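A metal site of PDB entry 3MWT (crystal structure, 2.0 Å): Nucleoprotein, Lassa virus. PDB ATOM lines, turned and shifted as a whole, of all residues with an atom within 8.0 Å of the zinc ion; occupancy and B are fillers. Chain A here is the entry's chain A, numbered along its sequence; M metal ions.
O of His 439 sits at hydrogen-bond distance from ND1 of His 517 (2.5 Å). A ring nitrogen (ND1) of His 517 sits close to the backbone carbonyl oxygen (O) of His 536 (3.3 Å). The side-chain carboxylate (OE1) of Glu 407 is in hydrogen-bond range of the backbone NH (N) of Ala 538, 3.0 Å away. The side-chain sulfur of Cys 537 lies close to the backbone NH of Leu 539 (3.6 Å). The backbone carbonyl oxygen (O) of Glu 407 lies within hydrogen-bond range of the backbone NH (N) of Glu 399 (2.8 Å). The backbone carbonyl oxygen (O) of Cys 514 lies within hydrogen-bond range of the side-chain amino group (NZ) of Lys 511, at 3.2 Å. N of Met 540 sits close to SG of Cys 537 (3.6 Å).
His 420 touches the zinc ion. Within 4 Å of the zinc ion: Glu 407, His 420, Cys 514, His 517 and Cys 537.
The zinc ion is bound by the side-chain sulfur (SG) of Cys 514 (2.0 Å), a ring nitrogen (NE2) of His 517 (2.2 Å), the side-chain sulfur (SG) of Cys 537 (2.2 Å) and the side-chain carboxylate (OE2) of Glu 407 (2.3 Å).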
ATOM      1  N   GLU A 399      17.163 -27.987  24.090  1.00  0.00           N
ATOM      2  CA  GLU A 399      17.742 -27.416  22.882  1.00  0.00           C
ATOM      3  C   GLU A 399      19.201 -27.685  22.931  1.00  0.00           C
ATOM      4  O   GLU A 399      19.809 -27.732  23.997  1.00  0.00           O
ATOM      5  CB  GLU A 399      17.435 -25.935  22.760  1.00  0.00           C
ATOM      6  CG  GLU A 399      15.984 -25.691  22.346  1.00  0.00           C
ATOM      7  CD  GLU A 399      15.761 -26.121  20.916  1.00  0.00           C
ATOM      8  OE1 GLU A 399      16.672 -25.876  20.095  1.00  0.00           O
ATOM      9  OE2 GLU A 399      14.708 -26.714  20.601  1.00  0.00           O
ATOM     10  N   GLU A 407      19.996 -25.695  26.507  1.00  0.00           N
ATOM     11  CA  GLU A 407      18.780 -25.210  27.217  1.00  0.00           C
ATOM     12  C   GLU A 407      17.849 -26.359  27.601  1.00  0.00           C
ATOM     13  O   GLU A 407      17.513 -27.202  26.767  1.00  0.00           O
ATOM     14  CB  GLU A 407      17.973 -24.190  26.401  1.00  0.00           C
ATOM     15  CG  GLU A 407      16.695 -23.797  27.110  1.00  0.00           C
ATOM     16  CD  GLU A 407      15.813 -22.862  26.309  1.00  0.00           C
ATOM     17  OE1 GLU A 407      15.654 -22.990  25.062  1.00  0.00           O
ATOM     18  OE2 GLU A 407      15.291 -21.990  27.002  1.00  0.00           O
ATOM     19  N   ILE A 408      17.377 -26.371  28.842  1.00  0.00           N
ATOM     20  CA  ILE A 408      16.613 -27.526  29.336  1.00  0.00           C
ATOM     21  C   ILE A 408      15.350 -27.050  30.010  1.00  0.00           C
ATOM     22  O   ILE A 408      15.394 -26.114  30.780  1.00  0.00           O
ATOM     23  CB  ILE A 408      17.445 -28.282  30.451  1.00  0.00           C
ATOM     24  CG1 ILE A 408      18.715 -28.880  29.877  1.00  0.00           C
ATOM     25  CG2 ILE A 408      16.615 -29.395  31.088  1.00  0.00           C
ATOM     26  CD1 ILE A 408      18.458 -29.816  28.771  1.00  0.00           C
ATOM     27  N   ALA A 409      14.241 -27.739  29.770  1.00  0.00           N
ATOM     28  CA  ALA A 409      13.026 -27.436  30.509  1.00  0.00           C
ATOM     29  C   ALA A 409      12.262 -28.674  30.969  1.00  0.00           C
ATOM     30  O   ALA A 409      12.286 -29.699  30.284  1.00  0.00           O
ATOM     31  CB  ALA A 409      12.149 -26.566  29.696  1.00  0.00           C
ATOM     32  N   HIS A 420      13.828 -24.352  34.339  1.00  0.00           N
ATOM     33  CA  HIS A 420      14.306 -23.871  33.065  1.00  0.00           C
ATOM     34  C   HIS A 420      15.674 -23.311  33.277  1.00  0.00           C
ATOM     35  O   HIS A 420      15.850 -22.448  34.108  1.00  0.00           O
ATOM     36  CB  HIS A 420      13.367 -22.783  32.537  1.00  0.00           C
ATOM     37  CG  HIS A 420      13.753 -22.224  31.213  1.00  0.00           C
ATOM     38  ND1 HIS A 420      13.653 -20.888  30.931  1.00  0.00           N
ATOM     39  CD2 HIS A 420      14.243 -22.803  30.100  1.00  0.00           C
ATOM     40  CE1 HIS A 420      14.075 -20.664  29.705  1.00  0.00           C
ATOM     41  NE2 HIS A 420      14.443 -21.810  29.168  1.00  0.00           N
ATOM     42  N   PHE A 421      16.641 -23.800  32.504  1.00  0.00           N
ATOM     43  CA  PHE A 421      18.003 -23.304  32.668  1.00  0.00           C
ATOM     44  C   PHE A 421      18.821 -23.527  31.407  1.00  0.00           C
ATOM     45  O   PHE A 421      18.352 -24.216  30.481  1.00  0.00           O
ATOM     46  CB  PHE A 421      18.691 -23.944  33.904  1.00  0.00           C
ATOM     47  CG  PHE A 421      18.794 -25.418  33.840  1.00  0.00           C
ATOM     48  CD1 PHE A 421      19.881 -26.033  33.216  1.00  0.00           C
ATOM     49  CD2 PHE A 421      17.798 -26.205  34.411  1.00  0.00           C
ATOM     50  CE1 PHE A 421      19.976 -27.423  33.141  1.00  0.00           C
ATOM     51  CE2 PHE A 421      17.887 -27.603  34.335  1.00  0.00           C
ATOM     52  CZ  PHE A 421      18.990 -28.218  33.705  1.00  0.00           C
ATOM     53  N   PHE A 422      20.050 -23.007  31.417  1.00  0.00           N
ATOM     54  CA  PHE A 422      20.938 -22.982  30.250  1.00  0.00           C
ATOM     55  C   PHE A 422      22.338 -23.594  30.514  1.00  0.00           C
ATOM     56  O   PHE A 422      22.692 -23.850  31.643  1.00  0.00           O
ATOM     57  CB  PHE A 422      21.106 -21.549  29.742  1.00  0.00           C
ATOM     58  CG  PHE A 422      19.802 -20.837  29.510  1.00  0.00           C
ATOM     59  CD1 PHE A 422      19.153 -20.947  28.266  1.00  0.00           C
ATOM     60  CD2 PHE A 422      19.220 -20.096  30.513  1.00  0.00           C
ATOM     61  CE1 PHE A 422      17.936 -20.277  28.036  1.00  0.00           C
ATOM     62  CE2 PHE A 422      17.986 -19.412  30.287  1.00  0.00           C
ATOM     63  CZ  PHE A 422      17.342 -19.532  29.077  1.00  0.00           C
ATOM     64  N   HIS A 439      17.397 -22.690  17.640  1.00  0.00           N
ATOM     65  CA  HIS A 439      17.123 -22.007  18.900  1.00  0.00           C
ATOM     66  C   HIS A 439      17.380 -20.497  18.922  1.00  0.00           C
ATOM     67  O   HIS A 439      16.938 -19.800  19.860  1.00  0.00           O
ATOM     68  CB  HIS A 439      17.779 -22.765  20.074  1.00  0.00           C
ATOM     69  CG  HIS A 439      19.234 -23.058  19.891  1.00  0.00           C
ATOM     70  ND1 HIS A 439      20.160 -22.080  19.574  1.00  0.00           N
ATOM     71  CD2 HIS A 439      19.928 -24.216  19.951  1.00  0.00           C
ATOM     72  CE1 HIS A 439      21.363 -22.618  19.511  1.00  0.00           C
ATOM     73  NE2 HIS A 439      21.247 -23.909  19.748  1.00  0.00           N
ATOM     74  N   ILE A 441      19.883 -18.774  19.696  1.00  0.00           N
ATOM     75  CA  ILE A 441      20.557 -18.264  20.856  1.00  0.00           C
ATOM     76  C   ILE A 441      21.942 -17.825  20.461  1.00  0.00           C
ATOM     77  O   ILE A 441      22.642 -18.535  19.727  1.00  0.00           O
ATOM     78  CB  ILE A 441      20.722 -19.355  21.929  1.00  0.00           C
ATOM     79  CG1 ILE A 441      19.375 -19.906  22.370  1.00  0.00           C
ATOM     80  CG2 ILE A 441      21.562 -18.835  23.102  1.00  0.00           C
ATOM     81  CD1 ILE A 441      19.514 -21.052  23.525  1.00  0.00           C
ATOM     82  N   TRP A 507       3.566 -18.419  23.054  1.00  0.00           N
ATOM     83  CA  TRP A 507       4.460 -17.220  23.023  1.00  0.00           C
ATOM     84  C   TRP A 507       3.701 -15.945  23.416  1.00  0.00           C
ATOM     85  O   TRP A 507       4.210 -15.140  24.217  1.00  0.00           O
ATOM     86  CB  TRP A 507       5.164 -17.047  21.642  1.00  0.00           C
ATOM     87  CG  TRP A 507       6.435 -17.913  21.485  1.00  0.00           C
ATOM     88  CD1 TRP A 507       6.591 -18.976  20.637  1.00  0.00           C
ATOM     89  CD2 TRP A 507       7.670 -17.787  22.204  1.00  0.00           C
ATOM     90  NE1 TRP A 507       7.853 -19.512  20.762  1.00  0.00           N
ATOM     91  CE2 TRP A 507       8.546 -18.806  21.708  1.00  0.00           C
ATOM     92  CE3 TRP A 507       8.123 -16.937  23.225  1.00  0.00           C
ATOM     93  CZ2 TRP A 507       9.827 -18.998  22.209  1.00  0.00           C
ATOM     94  CZ3 TRP A 507       9.425 -17.133  23.733  1.00  0.00           C
ATOM     95  CH2 TRP A 507      10.271 -18.134  23.183  1.00  0.00           C
ATOM     96  N   LYS A 511       5.860 -15.166  26.646  1.00  0.00           N
ATOM     97  CA  LYS A 511       7.100 -14.628  26.076  1.00  0.00           C
ATOM     98  C   LYS A 511       8.024 -14.105  27.149  1.00  0.00           C
ATOM     99  O   LYS A 511       9.233 -14.343  27.080  1.00  0.00           O
ATOM    100  CB  LYS A 511       6.781 -13.526  25.035  1.00  0.00           C
ATOM    101  CG  LYS A 511       7.957 -12.636  24.631  1.00  0.00           C
ATOM    102  CD  LYS A 511       9.130 -13.467  23.993  1.00  0.00           C
ATOM    103  CE  LYS A 511      10.382 -12.601  23.945  1.00  0.00           C
ATOM    104  NZ  LYS A 511      10.916 -12.399  25.322  1.00  0.00           N
ATOM    105  N   LEU A 513       8.757 -15.178  29.968  1.00  0.00           N
ATOM    106  CA  LEU A 513       9.481 -16.197  30.692  1.00  0.00           C
ATOM    107  C   LEU A 513      10.837 -16.619  30.033  1.00  0.00           C
ATOM    108  O   LEU A 513      11.612 -17.344  30.661  1.00  0.00           O
ATOM    109  CB  LEU A 513       8.604 -17.429  30.944  1.00  0.00           C
ATOM    110  CG  LEU A 513       7.256 -17.327  31.669  1.00  0.00           C
ATOM    111  CD1 LEU A 513       6.685 -18.746  31.862  1.00  0.00           C
ATOM    112  CD2 LEU A 513       7.379 -16.635  33.040  1.00  0.00           C
ATOM    113  N   CYS A 514      11.104 -16.197  28.789  1.00  0.00           N
ATOM    114  CA  CYS A 514      12.420 -16.536  28.193  1.00  0.00           C
ATOM    115  C   CYS A 514      12.833 -15.434  27.227  1.00  0.00           C
ATOM    116  O   CYS A 514      12.172 -15.218  26.233  1.00  0.00           O
ATOM    117  CB  CYS A 514      12.380 -17.897  27.456  1.00  0.00           C
ATOM    118  SG  CYS A 514      14.051 -18.721  26.942  1.00  0.00           S
ATOM    119  N   HIS A 515      13.976 -14.801  27.505  1.00  0.00           N
ATOM    120  CA  HIS A 515      14.556 -13.768  26.654  1.00  0.00           C
ATOM    121  C   HIS A 515      15.798 -14.197  25.863  1.00  0.00           C
ATOM    122  O   HIS A 515      16.479 -13.370  25.278  1.00  0.00           O
ATOM    123  CB  HIS A 515      14.844 -12.548  27.499  1.00  0.00           C
ATOM    124  CG  HIS A 515      13.610 -11.917  28.083  1.00  0.00           C
ATOM    125  ND1 HIS A 515      12.978 -10.837  27.489  1.00  0.00           N
ATOM    126  CD2 HIS A 515      12.885 -12.208  29.182  1.00  0.00           C
ATOM    127  CE1 HIS A 515      11.918 -10.508  28.203  1.00  0.00           C
ATOM    128  NE2 HIS A 515      11.835 -11.327  29.231  1.00  0.00           N
ATOM    129  N   MET A 516      16.050 -15.506  25.801  1.00  0.00           N
ATOM    130  CA  MET A 516      17.348 -15.992  25.351  1.00  0.00           C
ATOM    131  C   MET A 516      17.483 -16.085  23.827  1.00  0.00           C
ATOM    132  O   MET A 516      18.594 -16.177  23.298  1.00  0.00           O
ATOM    133  CB  MET A 516      17.688 -17.342  26.011  1.00  0.00           C
ATOM    134  CG  MET A 516      19.166 -17.777  25.818  1.00  0.00           C
ATOM    135  SD  MET A 516      20.457 -16.730  26.528  1.00  0.00           S
ATOM    136  CE  MET A 516      20.097 -16.743  28.284  1.00  0.00           C
ATOM    137  N   HIS A 517      16.333 -16.068  23.155  1.00  0.00           N
ATOM    138  CA  HIS A 517      16.234 -16.382  21.755  1.00  0.00           C
ATOM    139  C   HIS A 517      16.171 -15.078  20.927  1.00  0.00           C
ATOM    140  O   HIS A 517      15.123 -14.381  20.836  1.00  0.00           O
ATOM    141  CB  HIS A 517      15.013 -17.276  21.508  1.00  0.00           C
ATOM    142  CG  HIS A 517      15.005 -18.538  22.329  1.00  0.00           C
ATOM    143  ND1 HIS A 517      15.449 -19.735  21.833  1.00  0.00           N
ATOM    144  CD2 HIS A 517      14.530 -18.800  23.573  1.00  0.00           C
ATOM    145  CE1 HIS A 517      15.287 -20.678  22.741  1.00  0.00           C
ATOM    146  NE2 HIS A 517      14.715 -20.129  23.798  1.00  0.00           N
ATOM    147  N   PRO A 535      11.869 -19.115  16.645  1.00  0.00           N
ATOM    148  CA  PRO A 535      12.911 -19.933  17.296  1.00  0.00           C
ATOM    149  C   PRO A 535      12.303 -20.915  18.281  1.00  0.00           C
ATOM    150  O   PRO A 535      11.172 -20.672  18.831  1.00  0.00           O
ATOM    151  CB  PRO A 535      13.740 -18.909  18.055  1.00  0.00           C
ATOM    152  CG  PRO A 535      13.514 -17.559  17.317  1.00  0.00           C
ATOM    153  CD  PRO A 535      12.186 -17.672  16.651  1.00  0.00           C
ATOM    154  N   HIS A 536      13.042 -22.005  18.498  1.00  0.00           N
ATOM    155  CA  HIS A 536      12.626 -23.095  19.398  1.00  0.00           C
ATOM    156  C   HIS A 536      13.180 -22.914  20.816  1.00  0.00           C
ATOM    157  O   HIS A 536      14.389 -22.741  21.034  1.00  0.00           O
ATOM    158  CB  HIS A 536      13.030 -24.464  18.821  1.00  0.00           C
ATOM    159  CG  HIS A 536      12.397 -24.776  17.496  1.00  0.00           C
ATOM    160  ND1 HIS A 536      12.782 -25.832  16.702  1.00  0.00           N
ATOM    161  CD2 HIS A 536      11.405 -24.144  16.816  1.00  0.00           C
ATOM    162  CE1 HIS A 536      12.043 -25.859  15.610  1.00  0.00           C
ATOM    163  NE2 HIS A 536      11.198 -24.844  15.661  1.00  0.00           N
ATOM    164  N   CYS A 537      12.267 -22.990  21.778  1.00  0.00           N
ATOM    165  CA  CYS A 537      12.608 -22.760  23.183  1.00  0.00           C
ATOM    166  C   CYS A 537      12.231 -24.051  23.883  1.00  0.00           C
ATOM    167  O   CYS A 537      11.137 -24.564  23.663  1.00  0.00           O
ATOM    168  CB  CYS A 537      11.806 -21.586  23.709  1.00  0.00           C
ATOM    169  SG  CYS A 537      11.952 -21.267  25.495  1.00  0.00           S
ATOM    170  N   ALA A 538      13.122 -24.600  24.680  1.00  0.00           N
ATOM    171  CA  ALA A 538      12.791 -25.831  25.422  1.00  0.00           C
ATOM    172  C   ALA A 538      11.507 -25.676  26.227  1.00  0.00           C
ATOM    173  O   ALA A 538      10.703 -26.623  26.315  1.00  0.00           O
ATOM    174  CB  ALA A 538      13.910 -26.196  26.362  1.00  0.00           C
ATOM    175  N   LEU A 539      11.376 -24.514  26.884  1.00  0.00           N
ATOM    176  CA  LEU A 539      10.296 -24.267  27.811  1.00  0.00           C
ATOM    177  C   LEU A 539       9.006 -24.067  27.052  1.00  0.00           C
ATOM    178  O   LEU A 539       8.051 -24.785  27.301  1.00  0.00           O
ATOM    179  CB  LEU A 539      10.584 -23.091  28.765  1.00  0.00           C
ATOM    180  CG  LEU A 539       9.398 -22.783  29.736  1.00  0.00           C
ATOM    181  CD1 LEU A 539       9.004 -23.984  30.592  1.00  0.00           C
ATOM    182  CD2 LEU A 539       9.684 -21.530  30.619  1.00  0.00           C
ATOM    183  N   MET A 540       8.989 -23.176  26.048  1.00  0.00           N
ATOM    184  CA  MET A 540       7.750 -22.977  25.296  1.00  0.00           C
ATOM    185  C   MET A 540       7.302 -24.263  24.605  1.00  0.00           C
ATOM    186  O   MET A 540       6.128 -24.510  24.449  1.00  0.00           O
ATOM    187  CB  MET A 540       7.871 -21.836  24.291  1.00  0.00           C
ATOM    188  CG  MET A 540       8.236 -20.484  24.884  1.00  0.00           C
ATOM    189  SD  MET A 540       7.144 -19.922  26.200  1.00  0.00           S
ATOM    190  CE  MET A 540       8.301 -19.142  27.326  1.00  0.00           C
ATOM    191  N   ASP A 541       8.248 -25.098  24.210  1.00  0.00           N
ATOM    192  CA  ASP A 541       7.944 -26.363  23.576  1.00  0.00           C
ATOM    193  C   ASP A 541       7.274 -27.323  24.559  1.00  0.00           C
ATOM    194  O   ASP A 541       6.312 -27.969  24.216  1.00  0.00           O
ATOM    195  CB  ASP A 541       9.202 -26.977  22.999  1.00  0.00           C
ATOM    196  CG  ASP A 541       9.599 -26.362  21.663  1.00  0.00           C
ATOM    197  OD1 ASP A 541       8.891 -25.442  21.165  1.00  0.00           O
ATOM    198  OD2 ASP A 541      10.612 -26.804  21.102  1.00  0.00           O
HETATM  199 ZN    ZN M   1      13.996 -20.436  25.865  1.00  0.00          ZN
